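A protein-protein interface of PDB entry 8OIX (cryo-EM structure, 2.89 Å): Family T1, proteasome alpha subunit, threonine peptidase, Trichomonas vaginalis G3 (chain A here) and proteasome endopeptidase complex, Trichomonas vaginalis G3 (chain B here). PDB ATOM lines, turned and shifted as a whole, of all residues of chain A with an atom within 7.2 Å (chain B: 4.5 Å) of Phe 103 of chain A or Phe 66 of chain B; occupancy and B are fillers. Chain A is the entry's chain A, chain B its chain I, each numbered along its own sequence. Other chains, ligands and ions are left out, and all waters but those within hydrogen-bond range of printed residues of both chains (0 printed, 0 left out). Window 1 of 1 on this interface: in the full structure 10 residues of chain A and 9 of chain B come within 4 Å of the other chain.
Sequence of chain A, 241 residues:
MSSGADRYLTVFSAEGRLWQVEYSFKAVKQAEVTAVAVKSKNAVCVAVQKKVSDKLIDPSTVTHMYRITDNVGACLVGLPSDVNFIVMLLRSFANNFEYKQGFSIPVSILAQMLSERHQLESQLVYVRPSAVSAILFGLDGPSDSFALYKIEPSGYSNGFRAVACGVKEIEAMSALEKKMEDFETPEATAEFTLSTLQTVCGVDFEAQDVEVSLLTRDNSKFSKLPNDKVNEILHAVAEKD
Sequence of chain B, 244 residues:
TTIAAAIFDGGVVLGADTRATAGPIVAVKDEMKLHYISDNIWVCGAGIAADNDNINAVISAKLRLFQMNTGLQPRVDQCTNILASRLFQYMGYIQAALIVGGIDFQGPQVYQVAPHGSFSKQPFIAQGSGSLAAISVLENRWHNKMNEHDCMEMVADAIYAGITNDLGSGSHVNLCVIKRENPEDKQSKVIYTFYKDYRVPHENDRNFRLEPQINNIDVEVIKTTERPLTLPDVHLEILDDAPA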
ATOM      1  N   ALA A  94      -9.925 -11.536 -29.170  1.00  0.00           N
ATOM      2  CA  ALA A  94     -11.221 -11.161 -28.623  1.00  0.00           C
ATOM      3  C   ALA A  94     -12.357 -11.857 -29.356  1.00  0.00           C
ATOM      4  O   ALA A  94     -13.310 -12.332 -28.730  1.00  0.00           O
ATOM      5  CB  ALA A  94     -11.383  -9.647 -28.698  1.00  0.00           C
ATOM      6  N   ASN A  95     -12.276 -11.929 -30.685  1.00  0.00           N
ATOM      7  CA  ASN A  95     -13.334 -12.575 -31.454  1.00  0.00           C
ATOM      8  C   ASN A  95     -13.369 -14.073 -31.202  1.00  0.00           C
ATOM      9  O   ASN A  95     -14.448 -14.654 -31.062  1.00  0.00           O
ATOM     10  CB  ASN A  95     -13.159 -12.293 -32.940  1.00  0.00           C
ATOM     11  CG  ASN A  95     -12.969 -10.833 -33.229  1.00  0.00           C
ATOM     12  OD1 ASN A  95     -13.176  -9.984 -32.362  1.00  0.00           O
ATOM     13  ND2 ASN A  95     -12.580 -10.522 -34.451  1.00  0.00           N
ATOM     14  N   ASN A  96     -12.202 -14.717 -31.156  1.00  0.00           N
ATOM     15  CA  ASN A  96     -12.169 -16.144 -30.860  1.00  0.00           C
ATOM     16  C   ASN A  96     -12.701 -16.420 -29.460  1.00  0.00           C
ATOM     17  O   ASN A  96     -13.452 -17.381 -29.249  1.00  0.00           O
ATOM     18  CB  ASN A  96     -10.743 -16.670 -31.022  1.00  0.00           C
ATOM     19  CG  ASN A  96     -10.660 -18.177 -30.915  1.00  0.00           C
ATOM     20  OD1 ASN A  96     -10.075 -18.713 -29.975  1.00  0.00           O
ATOM     21  ND2 ASN A  96     -11.246 -18.872 -31.883  1.00  0.00           N
ATOM     22  N   PHE A  97     -12.345 -15.570 -28.496  1.00  0.00           N
ATOM     23  CA  PHE A  97     -12.843 -15.735 -27.137  1.00  0.00           C
ATOM     24  C   PHE A  97     -14.351 -15.543 -27.074  1.00  0.00           C
ATOM     25  O   PHE A  97     -15.046 -16.284 -26.375  1.00  0.00           O
ATOM     26  CB  PHE A  97     -12.131 -14.763 -26.197  1.00  0.00           C
ATOM     27  CG  PHE A  97     -12.493 -14.939 -24.752  1.00  0.00           C
ATOM     28  CD1 PHE A  97     -13.626 -14.346 -24.226  1.00  0.00           C
ATOM     29  CD2 PHE A  97     -11.703 -15.710 -23.922  1.00  0.00           C
ATOM     30  CE1 PHE A  97     -13.958 -14.512 -22.903  1.00  0.00           C
ATOM     31  CE2 PHE A  97     -12.034 -15.880 -22.597  1.00  0.00           C
ATOM     32  CZ  PHE A  97     -13.162 -15.279 -22.087  1.00  0.00           C
ATOM     33  N   GLU A  98     -14.877 -14.539 -27.774  1.00  0.00           N
ATOM     34  CA  GLU A  98     -16.318 -14.318 -27.759  1.00  0.00           C
ATOM     35  C   GLU A  98     -17.057 -15.430 -28.491  1.00  0.00           C
ATOM     36  O   GLU A  98     -18.187 -15.766 -28.126  1.00  0.00           O
ATOM     37  CB  GLU A  98     -16.648 -12.954 -28.365  1.00  0.00           C
ATOM     38  CG  GLU A  98     -18.134 -12.696 -28.551  1.00  0.00           C
ATOM     39  CD  GLU A  98     -18.471 -11.221 -28.593  1.00  0.00           C
ATOM     40  OE1 GLU A  98     -18.569 -10.601 -27.513  1.00  0.00           O
ATOM     41  OE2 GLU A  98     -18.639 -10.680 -29.705  1.00  0.00           O
ATOM     42  N   TYR A  99     -16.444 -16.011 -29.521  1.00  0.00           N
ATOM     43  CA  TYR A  99     -17.085 -17.110 -30.231  1.00  0.00           C
ATOM     44  C   TYR A  99     -17.102 -18.378 -29.388  1.00  0.00           C
ATOM     45  O   TYR A  99     -18.072 -19.143 -29.429  1.00  0.00           O
ATOM     46  CB  TYR A  99     -16.381 -17.355 -31.564  1.00  0.00           C
ATOM     47  CG  TYR A  99     -16.973 -18.490 -32.364  1.00  0.00           C
ATOM     48  CD1 TYR A  99     -18.176 -18.335 -33.037  1.00  0.00           C
ATOM     49  CD2 TYR A  99     -16.330 -19.716 -32.447  1.00  0.00           C
ATOM     50  CE1 TYR A  99     -18.723 -19.368 -33.768  1.00  0.00           C
ATOM     51  CE2 TYR A  99     -16.869 -20.755 -33.177  1.00  0.00           C
ATOM     52  CZ  TYR A  99     -18.066 -20.576 -33.836  1.00  0.00           C
ATOM     53  OH  TYR A  99     -18.606 -21.610 -34.565  1.00  0.00           O
ATOM     54  N   LYS A 100     -16.039 -18.622 -28.618  1.00  0.00           N
ATOM     55  CA  LYS A 100     -15.981 -19.834 -27.808  1.00  0.00           C
ATOM     56  C   LYS A 100     -16.740 -19.671 -26.494  1.00  0.00           C
ATOM     57  O   LYS A 100     -17.709 -20.388 -26.229  1.00  0.00           O
ATOM     58  CB  LYS A 100     -14.525 -20.212 -27.530  1.00  0.00           C
ATOM     59  CG  LYS A 100     -13.706 -20.528 -28.762  1.00  0.00           C
ATOM     60  CD  LYS A 100     -12.278 -20.861 -28.375  1.00  0.00           C
ATOM     61  CE  LYS A 100     -11.680 -19.757 -27.514  1.00  0.00           C
ATOM     62  NZ  LYS A 100     -10.194 -19.822 -27.473  1.00  0.00           N
ATOM     63  N   GLN A 101     -16.306 -18.725 -25.661  1.00  0.00           N
ATOM     64  CA  GLN A 101     -16.911 -18.491 -24.356  1.00  0.00           C
ATOM     65  C   GLN A 101     -18.248 -17.766 -24.432  1.00  0.00           C
ATOM     66  O   GLN A 101     -18.997 -17.783 -23.452  1.00  0.00           O
ATOM     67  CB  GLN A 101     -15.953 -17.686 -23.477  1.00  0.00           C
ATOM     68  CG  GLN A 101     -14.968 -18.525 -22.683  1.00  0.00           C
ATOM     69  CD  GLN A 101     -13.986 -19.267 -23.560  1.00  0.00           C
ATOM     70  OE1 GLN A 101     -13.697 -18.850 -24.680  1.00  0.00           O
ATOM     71  NE2 GLN A 101     -13.466 -20.378 -23.055  1.00  0.00           N
ATOM     72  N   GLY A 102     -18.562 -17.125 -25.552  1.00  0.00           N
ATOM     73  CA  GLY A 102     -19.851 -16.487 -25.708  1.00  0.00           C
ATOM     74  C   GLY A 102     -19.974 -15.098 -25.122  1.00  0.00           C
ATOM     75  O   GLY A 102     -21.057 -14.506 -25.207  1.00  0.00           O
ATOM     76  N   PHE A 103     -18.912 -14.552 -24.530  1.00  0.00           N
ATOM     77  CA  PHE A 103     -18.959 -13.208 -23.974  1.00  0.00           C
ATOM     78  C   PHE A 103     -17.670 -12.472 -24.307  1.00  0.00           C
ATOM     79  O   PHE A 103     -16.635 -13.081 -24.586  1.00  0.00           O
ATOM     80  CB  PHE A 103     -19.203 -13.232 -22.458  1.00  0.00           C
ATOM     81  CG  PHE A 103     -18.066 -13.804 -21.660  1.00  0.00           C
ATOM     82  CD1 PHE A 103     -17.962 -15.167 -21.457  1.00  0.00           C
ATOM     83  CD2 PHE A 103     -17.121 -12.975 -21.082  1.00  0.00           C
ATOM     84  CE1 PHE A 103     -16.926 -15.692 -20.716  1.00  0.00           C
ATOM     85  CE2 PHE A 103     -16.083 -13.496 -20.339  1.00  0.00           C
ATOM     86  CZ  PHE A 103     -15.987 -14.856 -20.155  1.00  0.00           C
ATOM     87  N   SER A 104     -17.755 -11.141 -24.288  1.00  0.00           N
ATOM     88  CA  SER A 104     -16.626 -10.302 -24.667  1.00  0.00           C
ATOM     89  C   SER A 104     -15.425 -10.577 -23.774  1.00  0.00           C
ATOM     90  O   SER A 104     -15.563 -10.777 -22.564  1.00  0.00           O
ATOM     91  CB  SER A 104     -17.013  -8.825 -24.587  1.00  0.00           C
ATOM     92  OG  SER A 104     -17.459  -8.486 -23.286  1.00  0.00           O
ATOM     93  N   ILE A 105     -14.243 -10.587 -24.381  1.00  0.00           N
ATOM     94  CA  ILE A 105     -13.037 -10.994 -23.653  1.00  0.00           C
ATOM     95  C   ILE A 105     -12.738  -9.990 -22.544  1.00  0.00           C
ATOM     96  O   ILE A 105     -12.842  -8.766 -22.762  1.00  0.00           O
ATOM     97  CB  ILE A 105     -11.843 -11.141 -24.616  1.00  0.00           C
ATOM     98  CG1 ILE A 105     -10.688 -11.864 -23.927  1.00  0.00           C
ATOM     99  CG2 ILE A 105     -11.383  -9.794 -25.150  1.00  0.00           C
ATOM    100  CD1 ILE A 105      -9.612 -12.309 -24.880  1.00  0.00           C
ATOM    101  N   PRO A 106     -12.436 -10.441 -21.332  1.00  0.00           N
ATOM    102  CA  PRO A 106     -11.957  -9.522 -20.298  1.00  0.00           C
ATOM    103  C   PRO A 106     -10.566  -9.004 -20.624  1.00  0.00           C
ATOM    104  O   PRO A 106      -9.801  -9.613 -21.374  1.00  0.00           O
ATOM    105  CB  PRO A 106     -11.947 -10.380 -19.028  1.00  0.00           C
ATOM    106  CG  PRO A 106     -12.822 -11.544 -19.338  1.00  0.00           C
ATOM    107  CD  PRO A 106     -12.701 -11.786 -20.802  1.00  0.00           C
ATOM    108  N   ILE A 109      -7.893 -11.543 -19.537  1.00  0.00           N
ATOM    109  CA  ILE A 109      -7.706 -12.685 -20.427  1.00  0.00           C
ATOM    110  C   ILE A 109      -7.040 -12.252 -21.725  1.00  0.00           C
ATOM    111  O   ILE A 109      -6.204 -12.974 -22.281  1.00  0.00           O
ATOM    112  CB  ILE A 109      -9.052 -13.380 -20.682  1.00  0.00           C
ATOM    113  CG1 ILE A 109      -9.653 -13.832 -19.354  1.00  0.00           C
ATOM    114  CG2 ILE A 109      -8.873 -14.562 -21.616  1.00  0.00           C
ATOM    115  CD1 ILE A 109     -10.917 -14.610 -19.500  1.00  0.00           C
ATOM    116  N   GLN A 112      -3.477 -11.926 -20.959  1.00  0.00           N
ATOM    117  CA  GLN A 112      -2.865 -13.248 -20.889  1.00  0.00           C
ATOM    118  C   GLN A 112      -2.599 -13.809 -22.280  1.00  0.00           C
ATOM    119  O   GLN A 112      -1.538 -14.390 -22.528  1.00  0.00           O
ATOM    120  CB  GLN A 112      -3.754 -14.200 -20.092  1.00  0.00           C
ATOM    121  CG  GLN A 112      -3.800 -13.912 -18.604  1.00  0.00           C
ATOM    122  CD  GLN A 112      -4.783 -14.802 -17.872  1.00  0.00           C
ATOM    123  OE1 GLN A 112      -5.666 -15.403 -18.482  1.00  0.00           O
ATOM    124  NE2 GLN A 112      -4.633 -14.892 -16.558  1.00  0.00           N
ATOM    125  N   PRO A 142     -17.825  -8.940 -14.864  1.00  0.00           N
ATOM    126  CA  PRO A 142     -17.897  -9.900 -13.747  1.00  0.00           C
ATOM    127  C   PRO A 142     -17.513  -9.297 -12.409  1.00  0.00           C
ATOM    128  O   PRO A 142     -18.099  -9.652 -11.379  1.00  0.00           O
ATOM    129  CB  PRO A 142     -16.927 -11.003 -14.182  1.00  0.00           C
ATOM    130  CG  PRO A 142     -17.000 -10.979 -15.656  1.00  0.00           C
ATOM    131  CD  PRO A 142     -17.161  -9.536 -16.039  1.00  0.00           C
ATOM    132  N   LYS B  62     -12.871 -27.631 -18.624  1.00  0.00           N
ATOM    133  CA  LYS B  62     -12.612 -26.397 -19.359  1.00  0.00           C
ATOM    134  C   LYS B  62     -12.802 -25.180 -18.468  1.00  0.00           C
ATOM    135  O   LYS B  62     -11.977 -24.263 -18.473  1.00  0.00           O
ATOM    136  CB  LYS B  62     -13.523 -26.304 -20.583  1.00  0.00           C
ATOM    137  CG  LYS B  62     -13.202 -27.298 -21.680  1.00  0.00           C
ATOM    138  CD  LYS B  62     -14.038 -27.031 -22.918  1.00  0.00           C
ATOM    139  CE  LYS B  62     -13.620 -27.930 -24.068  1.00  0.00           C
ATOM    140  NZ  LYS B  62     -12.166 -27.811 -24.365  1.00  0.00           N
ATOM    141  N   LEU B  63     -13.873 -25.161 -17.676  1.00  0.00           N
ATOM    142  CA  LEU B  63     -14.132 -24.011 -16.822  1.00  0.00           C
ATOM    143  C   LEU B  63     -13.255 -23.998 -15.579  1.00  0.00           C
ATOM    144  O   LEU B  63     -12.983 -22.920 -15.049  1.00  0.00           O
ATOM    145  CB  LEU B  63     -15.609 -23.954 -16.439  1.00  0.00           C
ATOM    146  CG  LEU B  63     -16.505 -23.670 -17.644  1.00  0.00           C
ATOM    147  CD1 LEU B  63     -17.957 -23.788 -17.270  1.00  0.00           C
ATOM    148  CD2 LEU B  63     -16.213 -22.293 -18.207  1.00  0.00           C
ATOM    149  N   ARG B  64     -12.764 -25.153 -15.132  1.00  0.00           N
ATOM    150  CA  ARG B  64     -11.794 -25.159 -14.044  1.00  0.00           C
ATOM    151  C   ARG B  64     -10.456 -24.632 -14.537  1.00  0.00           C
ATOM    152  O   ARG B  64      -9.788 -23.860 -13.842  1.00  0.00           O
ATOM    153  CB  ARG B  64     -11.652 -26.570 -13.472  1.00  0.00           C
ATOM    154  CG  ARG B  64     -10.314 -26.850 -12.807  1.00  0.00           C
ATOM    155  CD  ARG B  64     -10.322 -28.195 -12.098  1.00  0.00           C
ATOM    156  NE  ARG B  64     -10.640 -28.073 -10.680  1.00  0.00           N
ATOM    157  CZ  ARG B  64      -9.884 -27.454  -9.783  1.00  0.00           C
ATOM    158  NH1 ARG B  64      -8.622 -27.146 -10.035  1.00  0.00           N
ATOM    159  NH2 ARG B  64     -10.379 -27.218  -8.571  1.00  0.00           N
ATOM    160  N   LEU B  65     -10.081 -24.997 -15.763  1.00  0.00           N
ATOM    161  CA  LEU B  65      -8.870 -24.460 -16.369  1.00  0.00           C
ATOM    162  C   LEU B  65      -9.022 -22.968 -16.623  1.00  0.00           C
ATOM    163  O   LEU B  65      -8.070 -22.199 -16.453  1.00  0.00           O
ATOM    164  CB  LEU B  65      -8.586 -25.211 -17.670  1.00  0.00           C
ATOM    165  CG  LEU B  65      -7.298 -24.957 -18.443  1.00  0.00           C
ATOM    166  CD1 LEU B  65      -6.112 -25.143 -17.541  1.00  0.00           C
ATOM    167  CD2 LEU B  65      -7.216 -25.897 -19.633  1.00  0.00           C
ATOM    168  N   PHE B  66     -10.229 -22.543 -16.996  1.00  0.00           N
ATOM    169  CA  PHE B  66     -10.520 -21.129 -17.187  1.00  0.00           C
ATOM    170  C   PHE B  66     -10.364 -20.372 -15.873  1.00  0.00           C
ATOM    171  O   PHE B  66      -9.672 -19.353 -15.806  1.00  0.00           O
ATOM    172  CB  PHE B  66     -11.933 -20.985 -17.757  1.00  0.00           C
ATOM    173  CG  PHE B  66     -12.391 -19.567 -17.922  1.00  0.00           C
ATOM    174  CD1 PHE B  66     -12.147 -18.888 -19.101  1.00  0.00           C
ATOM    175  CD2 PHE B  66     -13.092 -18.925 -16.917  1.00  0.00           C
ATOM    176  CE1 PHE B  66     -12.575 -17.592 -19.267  1.00  0.00           C
ATOM    177  CE2 PHE B  66     -13.519 -17.626 -17.076  1.00  0.00           C
ATOM    178  CZ  PHE B  66     -13.261 -16.958 -18.253  1.00  0.00           C
ATOM    179  N   GLN B  67     -11.033 -20.846 -14.819  1.00  0.00           N
ATOM    180  CA  GLN B  67     -10.963 -20.185 -13.524  1.00  0.00           C
ATOM    181  C   GLN B  67      -9.547 -20.198 -12.959  1.00  0.00           C
ATOM    182  O   GLN B  67      -9.170 -19.289 -12.212  1.00  0.00           O
ATOM    183  CB  GLN B  67     -11.931 -20.855 -12.547  1.00  0.00           C
ATOM    184  CG  GLN B  67     -11.933 -20.255 -11.152  1.00  0.00           C
ATOM    185  CD  GLN B  67     -13.290 -20.341 -10.487  1.00  0.00           C
ATOM    186  OE1 GLN B  67     -14.048 -21.281 -10.720  1.00  0.00           O
ATOM    187  NE2 GLN B  67     -13.606 -19.355  -9.656  1.00  0.00           N
ATOM    188  N   MET B  68      -8.748 -21.211 -13.298  1.00  0.00           N
ATOM    189  CA  MET B  68      -7.365 -21.240 -12.835  1.00  0.00           C
ATOM    190  C   MET B  68      -6.507 -20.226 -13.585  1.00  0.00           C
ATOM    191  O   MET B  68      -5.867 -19.365 -12.972  1.00  0.00           O
ATOM    192  CB  MET B  68      -6.792 -22.650 -12.979  1.00  0.00           C
ATOM    193  CG  MET B  68      -7.237 -23.605 -11.885  1.00  0.00           C
ATOM    194  SD  MET B  68      -6.324 -25.158 -11.883  1.00  0.00           S
ATOM    195  CE  MET B  68      -6.797 -25.830 -13.474  1.00  0.00           C
ATOM    196  N   ASN B  69      -6.475 -20.319 -14.917  1.00  0.00           N
ATOM    197  CA  ASN B  69      -5.632 -19.424 -15.704  1.00  0.00           C
ATOM    198  C   ASN B  69      -6.044 -17.968 -15.524  1.00  0.00           C
ATOM    199  O   ASN B  69      -5.199 -17.093 -15.307  1.00  0.00           O
ATOM    200  CB  ASN B  69      -5.684 -19.810 -17.182  1.00  0.00           C
ATOM    201  CG  ASN B  69      -5.316 -21.256 -17.420  1.00  0.00           C
ATOM    202  OD1 ASN B  69      -5.950 -21.947 -18.215  1.00  0.00           O
ATOM    203  ND2 ASN B  69      -4.284 -21.722 -16.733  1.00  0.00           N
ATOM    204  N   THR B  70      -7.342 -17.692 -15.609  1.00  0.00           N
ATOM    205  CA  THR B  70      -7.857 -16.333 -15.642  1.00  0.00           C
ATOM    206  C   THR B  70      -8.310 -15.817 -14.284  1.00  0.00           C
ATOM    207  O   THR B  70      -8.548 -14.613 -14.149  1.00  0.00           O
ATOM    208  CB  THR B  70      -9.025 -16.253 -16.627  1.00  0.00           C
ATOM    209  OG1 THR B  70     -10.168 -16.902 -16.061  1.00  0.00           O
ATOM    210  CG2 THR B  70      -8.659 -16.960 -17.920  1.00  0.00           C
ATOM    211  N   GLY B  71      -8.434 -16.684 -13.282  1.00  0.00           N
ATOM    212  CA  GLY B  71      -8.935 -16.256 -11.990  1.00  0.00           C
ATOM    213  C   GLY B  71     -10.367 -15.779 -11.998  1.00  0.00           C
ATOM    214  O   GLY B  71     -10.792 -15.106 -11.057  1.00  0.00           O
ATOM    215  N   LEU B  72     -11.127 -16.107 -13.038  1.00  0.00           N
ATOM    216  CA  LEU B  72     -12.482 -15.605 -13.204  1.00  0.00           C
ATOM    217  C   LEU B  72     -13.505 -16.690 -12.903  1.00  0.00           C
ATOM    218  O   LEU B  72     -13.312 -17.858 -13.250  1.00  0.00           O
ATOM    219  CB  LEU B  72     -12.696 -15.080 -14.623  1.00  0.00           C
ATOM    220  CG  LEU B  72     -11.850 -13.874 -15.020  1.00  0.00           C
ATOM    221  CD1 LEU B  72     -12.302 -13.357 -16.362  1.00  0.00           C
ATOM    222  CD2 LEU B  72     -11.939 -12.784 -13.968  1.00  0.00           C
ATOM    223  N   GLN B  73     -14.590 -16.292 -12.256  1.00  0.00           N
ATOM    224  CA  GLN B  73     -15.693 -17.208 -12.006  1.00  0.00           C
ATOM    225  C   GLN B  73     -16.345 -17.592 -13.329  1.00  0.00           C
ATOM    226  O   GLN B  73     -16.689 -16.705 -14.120  1.00  0.00           O
ATOM    227  CB  GLN B  73     -16.719 -16.564 -11.079  1.00  0.00           C
ATOM    228  CG  GLN B  73     -17.860 -17.476 -10.683  1.00  0.00           C
ATOM    229  CD  GLN B  73     -18.975 -16.731  -9.984  1.00  0.00           C
ATOM    230  OE1 GLN B  73     -19.407 -15.671 -10.437  1.00  0.00           O
ATOM    231  NE2 GLN B  73     -19.447 -17.279  -8.872  1.00  0.00           N
ATOM    232  N   ARG B  75     -18.997 -18.249 -16.087  1.00  0.00           N
ATOM    233  CA  ARG B  75     -20.316 -17.677 -16.294  1.00  0.00           C
ATOM    234  C   ARG B  75     -21.278 -18.741 -16.801  1.00  0.00           C
ATOM    235  O   ARG B  75     -20.892 -19.637 -17.557  1.00  0.00           O
ATOM    236  CB  ARG B  75     -20.249 -16.512 -17.280  1.00  0.00           C
ATOM    237  CG  ARG B  75     -19.567 -15.278 -16.727  1.00  0.00           C
ATOM    238  CD  ARG B  75     -19.284 -14.266 -17.817  1.00  0.00           C
ATOM    239  NE  ARG B  75     -20.483 -13.944 -18.580  1.00  0.00           N
ATOM    240  CZ  ARG B  75     -20.625 -12.858 -19.326  1.00  0.00           C
ATOM    241  NH1 ARG B  75     -19.673 -11.943 -19.402  1.00  0.00           N
ATOM    242  NH2 ARG B  75     -21.754 -12.681 -20.005  1.00  0.00           N
ATOM    243  N   GLN B  78     -21.476 -18.470 -20.298  1.00  0.00           N
ATOM    244  CA  GLN B  78     -20.230 -19.000 -20.848  1.00  0.00           C
ATOM    245  C   GLN B  78     -20.262 -20.522 -20.917  1.00  0.00           C
ATOM    246  O   GLN B  78     -19.937 -21.116 -21.954  1.00  0.00           O
ATOM    247  CB  GLN B  78     -19.048 -18.533 -20.003  1.00  0.00           C
ATOM    248  CG  GLN B  78     -17.731 -19.192 -20.355  1.00  0.00           C
ATOM    249  CD  GLN B  78     -16.621 -18.810 -19.402  1.00  0.00           C
ATOM    250  OE1 GLN B  78     -16.814 -17.992 -18.504  1.00  0.00           O
ATOM    251  NE2 GLN B  78     -15.451 -19.399 -19.592  1.00  0.00           N
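The side-chain amide nitrogen (NE2) of Gln 112 of chain A lies within hydrogen-bond range of the backbone carbonyl oxygen (O) of Asn 69 of chain B.
O of Phe 97 of chain A lies close to OE1 of Gln 101 of chain A. The backbone carbonyl oxygen (O) of Leu 65 of chain B lies close to the side-chain amide oxygen (OD1) of Asn 69 of chain B, at 2.8 Å. The backbone carbonyl oxygen (O) of Phe 66 of chain B is in hydrogen-bond range of the side-chain hydroxyl (OG1) of Thr 70 of chain B, at 2.5 Å. OG1 of Thr 70 of chain B sits close to N of Leu 72 of chain B, at 3.3 Å. OE1 of Gln 78 of chain B sits at hydrogen-bond distance from N of Arg 75 of chain B (3.3 Å).
Among the printed residues, pairs that only touch across the chains: Gln 101 of chain A with Gln 78 of chain B (3.1 Å), Phe 103 of chain A with Gln 78 of chain B (3.2 Å), Phe 103 of chain A with Arg 75 of chain B (3.2 Å), Ile 109 of chain A with Phe 66 of chain B (3.4 Å), Gln 112 of chain A with Thr 70 of chain B (3.4 Å), Pro 106 of chain A with Leu 72 of chain B (3.5 Å), Ile 109 of chain A with Thr 70 of chain B (3.6 Å), Ile 109 of chain A with Leu 72 of chain B (3.7 Å), Phe 97 of chain A with Phe 66 of chain B (3.7 Å) and Phe 103 of chain A with Phe 66 of chain B (3.9 Å).
Of the printed residues of chain B, Phe 97 of chain A touches Phe 66. Of the printed residues of chain B, Gln 101 of chain A touches Gln 78 (3.1 Å). Phe 103 of chain A touches just these residues of chain B: Phe 66, Arg 75 and Gln 78. Printed residues of chain B within 4 Å of Gln 112 of chain A: Asn 69 (2.6 Å) and Thr 70 (3.4 Å). Of chain A, only Phe 97 (3.7 Å), Phe 103 (3.9 Å) and Ile 109 (3.4 Å) come within 4 Å of Phe 66 of chain B. The nearest printed residue of chain B that does not touch Phe 103 of chain A is Leu 72 of chain B (5.5 Å). The nearest printed residue of chain A that does not touch Leu 72 of chain B is Pro 142 of chain A (5.3 Å).
Printed residues of chain B that touch a printed residue of chain A: Phe 66, Asn 69, Thr 70, Leu 72, Arg 75 and Gln 78. Hydrophobic or aromatic side chains of chain B that line the printed part of chain A: Phe 66 and Leu 72. Hydrophobic or aromatic side chains of chain A that line the printed part of chain B: Phe 97, Phe 103, Pro 106 and Ile 109. Among the printed residues, 11 pairs touch across the chains.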
